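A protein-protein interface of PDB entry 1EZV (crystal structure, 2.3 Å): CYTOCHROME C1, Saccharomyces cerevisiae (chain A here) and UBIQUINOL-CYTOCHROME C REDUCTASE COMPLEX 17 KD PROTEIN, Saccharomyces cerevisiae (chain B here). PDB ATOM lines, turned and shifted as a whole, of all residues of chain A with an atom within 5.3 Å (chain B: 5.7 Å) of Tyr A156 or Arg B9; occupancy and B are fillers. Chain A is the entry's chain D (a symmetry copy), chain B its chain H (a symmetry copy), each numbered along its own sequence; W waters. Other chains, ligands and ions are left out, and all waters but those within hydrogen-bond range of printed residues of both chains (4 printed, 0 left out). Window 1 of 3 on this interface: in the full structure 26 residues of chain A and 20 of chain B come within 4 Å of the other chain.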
ATOM      1  N   GLY A   7      34.712  20.103  14.716  1.00  0.00           N
ATOM      2  CA  GLY A   7      34.549  18.674  14.526  1.00  0.00           C
ATOM      3  C   GLY A   7      33.756  18.055  15.661  1.00  0.00           C
ATOM      4  O   GLY A   7      33.755  18.576  16.784  1.00  0.00           O
ATOM      5  N   LEU A   8      33.074  16.948  15.370  1.00  0.00           N
ATOM      6  CA  LEU A   8      32.254  16.263  16.366  1.00  0.00           C
ATOM      7  C   LEU A   8      33.132  15.608  17.422  1.00  0.00           C
ATOM      8  O   LEU A   8      34.102  14.923  17.103  1.00  0.00           O
ATOM      9  CB  LEU A   8      31.383  15.196  15.701  1.00  0.00           C
ATOM     10  CG  LEU A   8      29.919  15.034  16.126  1.00  0.00           C
ATOM     11  CD1 LEU A   8      29.555  13.575  16.060  1.00  0.00           C
ATOM     12  CD2 LEU A   8      29.671  15.570  17.518  1.00  0.00           C
ATOM     13  N   HIS A   9      32.791  15.842  18.681  1.00  0.00           N
ATOM     14  CA  HIS A   9      33.434  15.171  19.800  1.00  0.00           C
ATOM     15  C   HIS A   9      33.275  13.657  19.657  1.00  0.00           C
ATOM     16  O   HIS A   9      32.160  13.149  19.557  1.00  0.00           O
ATOM     17  CB  HIS A   9      32.801  15.646  21.116  1.00  0.00           C
ATOM     18  CG  HIS A   9      33.344  14.964  22.334  1.00  0.00           C
ATOM     19  ND1 HIS A   9      32.610  14.056  23.070  1.00  0.00           N
ATOM     20  CD2 HIS A   9      34.552  15.055  22.945  1.00  0.00           C
ATOM     21  CE1 HIS A   9      33.342  13.615  24.079  1.00  0.00           C
ATOM     22  NE2 HIS A   9      34.524  14.206  24.026  1.00  0.00           N
ATOM     23  N   ALA A  10      34.398  12.947  19.624  1.00  0.00           N
ATOM     24  CA  ALA A  10      34.386  11.494  19.628  1.00  0.00           C
ATOM     25  C   ALA A  10      33.994  10.981  21.012  1.00  0.00           C
ATOM     26  O   ALA A  10      34.441  11.511  22.026  1.00  0.00           O
ATOM     27  CB  ALA A  10      35.754  10.960  19.234  1.00  0.00           C
ATOM     28  N   PRO A  11      33.094   9.982  21.066  1.00  0.00           N
ATOM     29  CA  PRO A  11      32.633   9.386  22.322  1.00  0.00           C
ATOM     30  C   PRO A  11      33.640   8.381  22.863  1.00  0.00           C
ATOM     31  O   PRO A  11      34.523   7.923  22.130  1.00  0.00           O
ATOM     32  CB  PRO A  11      31.337   8.701  21.915  1.00  0.00           C
ATOM     33  CG  PRO A  11      31.627   8.238  20.534  1.00  0.00           C
ATOM     34  CD  PRO A  11      32.455   9.337  19.904  1.00  0.00           C
ATOM     35  N   TYR A  13      34.546   4.806  23.809  1.00  0.00           N
ATOM     36  CA  TYR A  13      34.330   3.362  23.693  1.00  0.00           C
ATOM     37  C   TYR A  13      35.073   2.598  24.786  1.00  0.00           C
ATOM     38  O   TYR A  13      36.051   3.098  25.345  1.00  0.00           O
ATOM     39  CB  TYR A  13      34.779   2.876  22.316  1.00  0.00           C
ATOM     40  CG  TYR A  13      33.892   3.373  21.203  1.00  0.00           C
ATOM     41  CD1 TYR A  13      32.603   2.860  21.037  1.00  0.00           C
ATOM     42  CD2 TYR A  13      34.302   4.407  20.362  1.00  0.00           C
ATOM     43  CE1 TYR A  13      31.741   3.370  20.069  1.00  0.00           C
ATOM     44  CE2 TYR A  13      33.443   4.926  19.388  1.00  0.00           C
ATOM     45  CZ  TYR A  13      32.162   4.405  19.253  1.00  0.00           C
ATOM     46  OH  TYR A  13      31.281   4.945  18.338  1.00  0.00           O
ATOM     47  N   TYR A 129      39.066   8.694  18.699  1.00  0.00           N
ATOM     48  CA  TYR A 129      39.010   9.533  17.513  1.00  0.00           C
ATOM     49  C   TYR A 129      39.204   8.696  16.253  1.00  0.00           C
ATOM     50  O   TYR A 129      38.374   8.732  15.358  1.00  0.00           O
ATOM     51  CB  TYR A 129      40.071  10.642  17.586  1.00  0.00           C
ATOM     52  CG  TYR A 129      40.238  11.399  16.294  1.00  0.00           C
ATOM     53  CD1 TYR A 129      39.207  12.199  15.795  1.00  0.00           C
ATOM     54  CD2 TYR A 129      41.380  11.242  15.519  1.00  0.00           C
ATOM     55  CE1 TYR A 129      39.306  12.808  14.547  1.00  0.00           C
ATOM     56  CE2 TYR A 129      41.495  11.857  14.273  1.00  0.00           C
ATOM     57  CZ  TYR A 129      40.450  12.635  13.795  1.00  0.00           C
ATOM     58  OH  TYR A 129      40.544  13.237  12.564  1.00  0.00           O
ATOM     59  N   SER A 132      36.281   6.385  15.552  1.00  0.00           N
ATOM     60  CA  SER A 132      35.107   7.153  15.175  1.00  0.00           C
ATOM     61  C   SER A 132      35.220   7.723  13.768  1.00  0.00           C
ATOM     62  O   SER A 132      34.254   7.702  13.008  1.00  0.00           O
ATOM     63  CB  SER A 132      34.864   8.272  16.186  1.00  0.00           C
ATOM     64  OG  SER A 132      34.322   7.755  17.392  1.00  0.00           O
ATOM     65  N   LEU A 133      36.415   8.162  13.395  1.00  0.00           N
ATOM     66  CA  LEU A 133      36.648   8.660  12.043  1.00  0.00           C
ATOM     67  C   LEU A 133      36.361   7.561  11.014  1.00  0.00           C
ATOM     68  O   LEU A 133      35.630   7.788  10.049  1.00  0.00           O
ATOM     69  CB  LEU A 133      38.094   9.153  11.889  1.00  0.00           C
ATOM     70  CG  LEU A 133      38.449   9.755  10.519  1.00  0.00           C
ATOM     71  CD1 LEU A 133      37.941  11.186  10.433  1.00  0.00           C
ATOM     72  CD2 LEU A 133      39.950   9.709  10.292  1.00  0.00           C
ATOM     73  N   THR A 135      34.596   4.861  11.146  1.00  0.00           N
ATOM     74  CA  THR A 135      33.252   4.309  11.151  1.00  0.00           C
ATOM     75  C   THR A 135      32.199   5.409  11.035  1.00  0.00           C
ATOM     76  O   THR A 135      31.004   5.164  11.220  1.00  0.00           O
ATOM     77  CB  THR A 135      32.992   3.528  12.446  1.00  0.00           C
ATOM     78  OG1 THR A 135      33.247   4.375  13.572  1.00  0.00           O
ATOM     79  CG2 THR A 135      33.891   2.307  12.523  1.00  0.00           C
ATOM     80  N   GLY A 136      32.640   6.618  10.710  1.00  0.00           N
ATOM     81  CA  GLY A 136      31.759   7.762  10.819  1.00  0.00           C
ATOM     82  C   GLY A 136      31.514   8.500   9.522  1.00  0.00           C
ATOM     83  O   GLY A 136      31.161   9.672   9.550  1.00  0.00           O
ATOM     84  N   ASN A 154      32.975  13.822   6.784  1.00  0.00           N
ATOM     85  CA  ASN A 154      33.105  13.037   7.999  1.00  0.00           C
ATOM     86  C   ASN A 154      32.966  14.016   9.153  1.00  0.00           C
ATOM     87  O   ASN A 154      33.702  15.003   9.224  1.00  0.00           O
ATOM     88  CB  ASN A 154      34.480  12.373   8.046  1.00  0.00           C
ATOM     89  CG  ASN A 154      34.562  11.291   9.089  1.00  0.00           C
ATOM     90  OD1 ASN A 154      34.262  11.520  10.265  1.00  0.00           O
ATOM     91  ND2 ASN A 154      34.977  10.101   8.673  1.00  0.00           N
ATOM     92  N   PRO A 155      31.971  13.806  10.029  1.00  0.00           N
ATOM     93  CA  PRO A 155      31.674  14.806  11.062  1.00  0.00           C
ATOM     94  C   PRO A 155      32.774  14.929  12.129  1.00  0.00           C
ATOM     95  O   PRO A 155      32.954  15.994  12.717  1.00  0.00           O
ATOM     96  CB  PRO A 155      30.353  14.317  11.647  1.00  0.00           C
ATOM     97  CG  PRO A 155      30.430  12.832  11.495  1.00  0.00           C
ATOM     98  CD  PRO A 155      31.134  12.603  10.179  1.00  0.00           C
ATOM     99  N   TYR A 156      33.555  13.868  12.319  1.00  0.00           N
ATOM    100  CA  TYR A 156      34.600  13.859  13.349  1.00  0.00           C
ATOM    101  C   TYR A 156      35.886  14.581  12.946  1.00  0.00           C
ATOM    102  O   TYR A 156      36.683  14.943  13.802  1.00  0.00           O
ATOM    103  CB  TYR A 156      34.919  12.422  13.759  1.00  0.00           C
ATOM    104  CG  TYR A 156      33.718  11.683  14.293  1.00  0.00           C
ATOM    105  CD1 TYR A 156      33.014  10.787  13.487  1.00  0.00           C
ATOM    106  CD2 TYR A 156      33.246  11.920  15.582  1.00  0.00           C
ATOM    107  CE1 TYR A 156      31.864  10.148  13.952  1.00  0.00           C
ATOM    108  CE2 TYR A 156      32.102  11.287  16.058  1.00  0.00           C
ATOM    109  CZ  TYR A 156      31.415  10.400  15.232  1.00  0.00           C
ATOM    110  OH  TYR A 156      30.290   9.767  15.690  1.00  0.00           O
ATOM    111  N   PHE A 157      36.078  14.799  11.649  1.00  0.00           N
ATOM    112  CA  PHE A 157      37.215  15.564  11.152  1.00  0.00           C
ATOM    113  C   PHE A 157      36.896  17.062  11.257  1.00  0.00           C
ATOM    114  O   PHE A 157      35.778  17.487  10.952  1.00  0.00           O
ATOM    115  CB  PHE A 157      37.487  15.188   9.696  1.00  0.00           C
ATOM    116  CG  PHE A 157      38.812  15.665   9.175  1.00  0.00           C
ATOM    117  CD1 PHE A 157      40.004  15.142   9.679  1.00  0.00           C
ATOM    118  CD2 PHE A 157      38.872  16.621   8.165  1.00  0.00           C
ATOM    119  CE1 PHE A 157      41.244  15.567   9.175  1.00  0.00           C
ATOM    120  CE2 PHE A 157      40.098  17.056   7.660  1.00  0.00           C
ATOM    121  CZ  PHE A 157      41.289  16.527   8.163  1.00  0.00           C
ATOM    122  N   PRO A 158      37.852  17.869  11.760  1.00  0.00           N
ATOM    123  CA  PRO A 158      37.673  19.324  11.851  1.00  0.00           C
ATOM    124  C   PRO A 158      37.377  19.933  10.496  1.00  0.00           C
ATOM    125  O   PRO A 158      38.126  19.726   9.546  1.00  0.00           O
ATOM    126  CB  PRO A 158      39.012  19.812  12.402  1.00  0.00           C
ATOM    127  CG  PRO A 158      39.522  18.648  13.188  1.00  0.00           C
ATOM    128  CD  PRO A 158      39.119  17.441  12.380  1.00  0.00           C
ATOM    129  N   GLN B   4      27.831  -4.163  13.538  1.00  0.00           N
ATOM    130  CA  GLN B   4      27.284  -4.057  14.886  1.00  0.00           C
ATOM    131  C   GLN B   4      26.977  -2.616  15.288  1.00  0.00           C
ATOM    132  O   GLN B   4      26.081  -2.367  16.096  1.00  0.00           O
ATOM    133  CB  GLN B   4      28.257  -4.677  15.891  1.00  0.00           C
ATOM    134  CG  GLN B   4      28.451  -6.183  15.744  1.00  0.00           C
ATOM    135  CD  GLN B   4      29.654  -6.563  14.889  1.00  0.00           C
ATOM    136  OE1 GLN B   4      30.272  -7.608  15.102  1.00  0.00           O
ATOM    137  NE2 GLN B   4      29.972  -5.735  13.900  1.00  0.00           N
ATOM    138  N   LEU B   5      27.741  -1.677  14.738  1.00  0.00           N
ATOM    139  CA  LEU B   5      27.524  -0.258  14.988  1.00  0.00           C
ATOM    140  C   LEU B   5      26.309   0.244  14.204  1.00  0.00           C
ATOM    141  O   LEU B   5      25.435   0.911  14.764  1.00  0.00           O
ATOM    142  CB  LEU B   5      28.775   0.541  14.598  1.00  0.00           C
ATOM    143  CG  LEU B   5      28.800   2.048  14.868  1.00  0.00           C
ATOM    144  CD1 LEU B   5      28.587   2.331  16.344  1.00  0.00           C
ATOM    145  CD2 LEU B   5      30.127   2.608  14.414  1.00  0.00           C
ATOM    146  N   GLU B   6      26.252  -0.105  12.920  1.00  0.00           N
ATOM    147  CA  GLU B   6      25.107   0.212  12.067  1.00  0.00           C
ATOM    148  C   GLU B   6      23.806  -0.304  12.669  1.00  0.00           C
ATOM    149  O   GLU B   6      22.765   0.348  12.574  1.00  0.00           O
ATOM    150  CB  GLU B   6      25.296  -0.405  10.681  1.00  0.00           C
ATOM    151  CG  GLU B   6      25.957   0.515   9.676  1.00  0.00           C
ATOM    152  CD  GLU B   6      25.117   0.702   8.427  1.00  0.00           C
ATOM    153  OE1 GLU B   6      25.286  -0.092   7.473  1.00  0.00           O
ATOM    154  OE2 GLU B   6      24.274   1.629   8.410  1.00  0.00           O
ATOM    155  N   ASP B   7      23.882  -1.482  13.283  1.00  0.00           N
ATOM    156  CA  ASP B   7      22.750  -2.101  13.959  1.00  0.00           C
ATOM    157  C   ASP B   7      22.276  -1.249  15.134  1.00  0.00           C
ATOM    158  O   ASP B   7      21.100  -0.897  15.215  1.00  0.00           O
ATOM    159  CB  ASP B   7      23.150  -3.495  14.453  1.00  0.00           C
ATOM    160  CG  ASP B   7      22.002  -4.236  15.118  1.00  0.00           C
ATOM    161  OD1 ASP B   7      21.333  -5.034  14.423  1.00  0.00           O
ATOM    162  OD2 ASP B   7      21.798  -4.052  16.340  1.00  0.00           O
ATOM    163  N   LEU B   8      23.199  -0.913  16.033  1.00  0.00           N
ATOM    164  CA  LEU B   8      22.883  -0.137  17.230  1.00  0.00           C
ATOM    165  C   LEU B   8      22.459   1.299  16.914  1.00  0.00           C
ATOM    166  O   LEU B   8      21.662   1.894  17.644  1.00  0.00           O
ATOM    167  CB  LEU B   8      24.079  -0.133  18.186  1.00  0.00           C
ATOM    168  CG  LEU B   8      24.198  -1.327  19.133  1.00  0.00           C
ATOM    169  CD1 LEU B   8      25.531  -1.284  19.853  1.00  0.00           C
ATOM    170  CD2 LEU B   8      23.057  -1.299  20.134  1.00  0.00           C
ATOM    171  N   ARG B   9      22.974   1.846  15.818  1.00  0.00           N
ATOM    172  CA  ARG B   9      22.560   3.168  15.374  1.00  0.00           C
ATOM    173  C   ARG B   9      21.114   3.150  14.881  1.00  0.00           C
ATOM    174  O   ARG B   9      20.271   3.883  15.399  1.00  0.00           O
ATOM    175  CB  ARG B   9      23.506   3.682  14.284  1.00  0.00           C
ATOM    176  CG  ARG B   9      24.634   4.541  14.843  1.00  0.00           C
ATOM    177  CD  ARG B   9      25.799   4.722  13.880  1.00  0.00           C
ATOM    178  NE  ARG B   9      26.898   5.423  14.544  1.00  0.00           N
ATOM    179  CZ  ARG B   9      28.042   5.780  13.966  1.00  0.00           C
ATOM    180  NH1 ARG B   9      28.940   6.463  14.666  1.00  0.00           N
ATOM    181  NH2 ARG B   9      28.297   5.456  12.703  1.00  0.00           N
ATOM    182  N   GLU B  10      20.809   2.207  13.989  1.00  0.00           N
ATOM    183  CA  GLU B  10      19.450   2.015  13.484  1.00  0.00           C
ATOM    184  C   GLU B  10      18.462   1.800  14.628  1.00  0.00           C
ATOM    185  O   GLU B  10      17.430   2.467  14.694  1.00  0.00           O
ATOM    186  CB  GLU B  10      19.407   0.820  12.524  1.00  0.00           C
ATOM    187  CG  GLU B  10      18.274   0.869  11.504  1.00  0.00           C
ATOM    188  CD  GLU B  10      18.259   2.163  10.699  1.00  0.00           C
ATOM    189  OE1 GLU B  10      19.336   2.581  10.211  1.00  0.00           O
ATOM    190  OE2 GLU B  10      17.171   2.770  10.566  1.00  0.00           O
ATOM    191  N   HIS B  11      18.843   0.962  15.585  1.00  0.00           N
ATOM    192  CA  HIS B  11      18.023   0.723  16.765  1.00  0.00           C
ATOM    193  C   HIS B  11      17.697   2.012  17.522  1.00  0.00           C
ATOM    194  O   HIS B  11      16.554   2.212  17.934  1.00  0.00           O
ATOM    195  CB  HIS B  11      18.718  -0.269  17.699  1.00  0.00           C
ATOM    196  CG  HIS B  11      18.084  -0.371  19.051  1.00  0.00           C
ATOM    197  ND1 HIS B  11      16.814  -0.874  19.241  1.00  0.00           N
ATOM    198  CD2 HIS B  11      18.516   0.028  20.270  1.00  0.00           C
ATOM    199  CE1 HIS B  11      16.489  -0.772  20.518  1.00  0.00           C
ATOM    200  NE2 HIS B  11      17.504  -0.228  21.165  1.00  0.00           N
ATOM    201  N   PHE B  12      18.685   2.896  17.674  1.00  0.00           N
ATOM    202  CA  PHE B  12      18.515   4.099  18.490  1.00  0.00           C
ATOM    203  C   PHE B  12      17.909   5.284  17.746  1.00  0.00           C
ATOM    204  O   PHE B  12      17.250   6.130  18.356  1.00  0.00           O
ATOM    205  CB  PHE B  12      19.841   4.498  19.150  1.00  0.00           C
ATOM    206  CG  PHE B  12      20.083   3.814  20.469  1.00  0.00           C
ATOM    207  CD1 PHE B  12      20.981   2.758  20.564  1.00  0.00           C
ATOM    208  CD2 PHE B  12      19.327   4.148  21.586  1.00  0.00           C
ATOM    209  CE1 PHE B  12      21.113   2.035  21.750  1.00  0.00           C
ATOM    210  CE2 PHE B  12      19.451   3.431  22.778  1.00  0.00           C
ATOM    211  CZ  PHE B  12      20.344   2.372  22.858  1.00  0.00           C
ATOM    212  N   LYS B  13      18.040   5.286  16.422  1.00  0.00           N
ATOM    213  CA  LYS B  13      17.287   6.219  15.586  1.00  0.00           C
ATOM    214  C   LYS B  13      15.770   6.058  15.765  1.00  0.00           C
ATOM    215  O   LYS B  13      15.006   6.985  15.485  1.00  0.00           O
ATOM    216  CB  LYS B  13      17.647   6.016  14.114  1.00  0.00           C
ATOM    217  CG  LYS B  13      19.011   6.541  13.732  1.00  0.00           C
ATOM    218  CD  LYS B  13      19.521   5.878  12.460  1.00  0.00           C
ATOM    219  CE  LYS B  13      19.936   6.912  11.430  1.00  0.00           C
ATOM    220  NZ  LYS B  13      18.808   7.832  11.100  1.00  0.00           N
ATOM    221  N   ASN B  14      15.347   4.895  16.259  1.00  0.00           N
ATOM    222  CA  ASN B  14      13.924   4.580  16.380  1.00  0.00           C
ATOM    223  C   ASN B  14      13.438   4.494  17.822  1.00  0.00           C
ATOM    224  O   ASN B  14      12.478   3.782  18.124  1.00  0.00           O
ATOM    225  CB  ASN B  14      13.602   3.275  15.637  1.00  0.00           C
ATOM    226  CG  ASN B  14      13.518   3.468  14.132  1.00  0.00           C
ATOM    227  OD1 ASN B  14      12.604   4.125  13.628  1.00  0.00           O
ATOM    228  ND2 ASN B  14      14.495   2.927  13.410  1.00  0.00           N
ATOM    229  N   GLN B  58      23.790  12.796  15.697  1.00  0.00           N
ATOM    230  CA  GLN B  58      24.990  11.983  15.837  1.00  0.00           C
ATOM    231  C   GLN B  58      25.483  11.918  17.278  1.00  0.00           C
ATOM    232  O   GLN B  58      25.908  10.859  17.744  1.00  0.00           O
ATOM    233  CB  GLN B  58      26.097  12.526  14.944  1.00  0.00           C
ATOM    234  CG  GLN B  58      27.131  11.490  14.588  1.00  0.00           C
ATOM    235  CD  GLN B  58      26.582  10.388  13.697  1.00  0.00           C
ATOM    236  OE1 GLN B  58      25.567  10.565  13.001  1.00  0.00           O
ATOM    237  NE2 GLN B  58      27.268   9.249  13.690  1.00  0.00           N
ATOM    238  N   LEU B  61      23.260   9.523  19.227  1.00  0.00           N
ATOM    239  CA  LEU B  61      23.588   8.164  18.820  1.00  0.00           C
ATOM    240  C   LEU B  61      24.923   7.695  19.408  1.00  0.00           C
ATOM    241  O   LEU B  61      25.014   6.585  19.942  1.00  0.00           O
ATOM    242  CB  LEU B  61      23.609   8.068  17.292  1.00  0.00           C
ATOM    243  CG  LEU B  61      22.277   8.385  16.592  1.00  0.00           C
ATOM    244  CD1 LEU B  61      22.474   8.355  15.078  1.00  0.00           C
ATOM    245  CD2 LEU B  61      21.198   7.386  17.025  1.00  0.00           C
ATOM    246  N   ASP B  62      25.923   8.574  19.387  1.00  0.00           N
ATOM    247  CA  ASP B  62      27.227   8.286  19.988  1.00  0.00           C
ATOM    248  C   ASP B  62      27.093   7.973  21.476  1.00  0.00           C
ATOM    249  O   ASP B  62      27.626   6.975  21.960  1.00  0.00           O
ATOM    250  CB  ASP B  62      28.176   9.474  19.803  1.00  0.00           C
ATOM    251  CG  ASP B  62      28.761   9.550  18.406  1.00  0.00           C
ATOM    252  OD1 ASP B  62      28.823   8.512  17.720  1.00  0.00           O
ATOM    253  OD2 ASP B  62      29.183  10.655  17.998  1.00  0.00           O
ATOM    254  N   THR B  65      25.395   4.467  21.704  1.00  0.00           N
ATOM    255  CA  THR B  65      26.065   3.331  21.077  1.00  0.00           C
ATOM    256  C   THR B  65      27.452   3.037  21.655  1.00  0.00           C
ATOM    257  O   THR B  65      27.851   1.877  21.765  1.00  0.00           O
ATOM    258  CB  THR B  65      26.196   3.532  19.552  1.00  0.00           C
ATOM    259  OG1 THR B  65      26.940   4.725  19.283  1.00  0.00           O
ATOM    260  CG2 THR B  65      24.826   3.643  18.910  1.00  0.00           C
HETATM  261  O   HOH W   1      31.944   6.770  13.971  1.00  0.00           O
HETATM  262  O   HOH W   2      28.706   9.995  10.986  1.00  0.00           O
HETATM  263  O   HOH W   3      31.459   7.195  16.736  1.00  0.00           O
HETATM  264  O   HOH W   4      29.751  12.246  20.288  1.00  0.00           O
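Leu A8 touches Gln B58 (CD1 to CG, 3.5 Å).
Asp B62 touches Leu A8.
CG of Pro A11 touches CB of Asp B62 (3.7 Å).
Leu B5 touches Thr A135 (CD2 to CB, 3.6 Å).
Tyr A156 touches Arg B9.
OH of Tyr A156 touches NE2 of Gln B58 (3.7 Å).
Water W1 lies within hydrogen-bond range of O of Ser A132 (2.7 Å), OG1 of Thr A135 (2.8 Å), NH1 of Arg B9 (3.1 Å) and N of Gly A136 (3.3 Å).
Water W4 bridges the backbone carbonyl oxygen (O) of His A9 (2.7 Å) and the side-chain carboxylate (OD2) of Asp B62 (2.8 Å).
Water W3 lies within hydrogen-bond range of the side-chain hydroxyl (OH) of Tyr A13 (2.8 Å), the side-chain hydroxyl (OG) of Ser A132 (3.0 Å), the side-chain hydroxyl (OH) of Tyr A156 (3.0 Å), the side-chain carboxylate (OD1) of Asp B62 (3.1 Å) and the guanidinium group (NH1) of Arg B9 (3.3 Å).
Water W2 lies within hydrogen-bond range of O of Gly A136 (2.9 Å) and NE2 of Gln B58 (3.2 Å).
O of Pro A155 is in hydrogen-bond range of N of Leu A8, at 2.8 Å.
OD1 of Asn A154 sits at hydrogen-bond distance from N of Tyr A156 (3.2 Å).
NH1 of Arg B9 sits close to NE2 of Gln B58, at 3.4 Å.
The guanidinium group (NH1) of Arg B9 is in salt-bridge range of the side-chain carboxylate (OD1) of Asp B62 (3.7 Å).
Of the 16 printed residues of chain A, 4 touch a printed residue of chain B.
Of the 15 printed residues of chain B, 4 touch a printed residue of chain A.
Hydrophobic or aromatic side chains of chain B within 4 Å of the printed part of chain A: Leu B5.
Among the printed residues, no Asp or Glu carboxylate lies within 4 Å of a Lys or Arg side-chain nitrogen of the other chain.
The backbone carbonyl oxygen (O) of Thr A135 lies within hydrogen-bond range of the guanidinium group (NH2) of Arg B9, at 3.1 Å.
The side-chain hydroxyl of Tyr A156 lies within hydrogen-bond range of the side-chain carboxylate of Asp B62 (2.7 Å).
Of the printed residues of chain B, Leu A8 touches Gln B58 and Asp B62.
Of the printed residues of chain B, Pro A11 touches Asp B62.
Tyr A156 touches just these residues of chain B: Arg B9 (3.7 Å), Gln B58 (3.7 Å) and Asp B62 (2.7 Å).
Of the printed residues of chain A, Leu B5 touches Thr A135.
Arg B9 touches two residues of chain A.
Of the printed residues of chain A, Gln B58 touches Leu A8 (3.5 Å) and Tyr A156 (3.7 Å).
Printed residues of chain A within 4 Å of Asp B62: Leu A8, Pro A11 and Tyr A156.
The nearest printed residue of chain B that does not touch Tyr A156 is Leu B61 (6.8 Å).
The nearest residue of chain A that does not touch Arg B9 is Gly A136 (4.6 Å).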
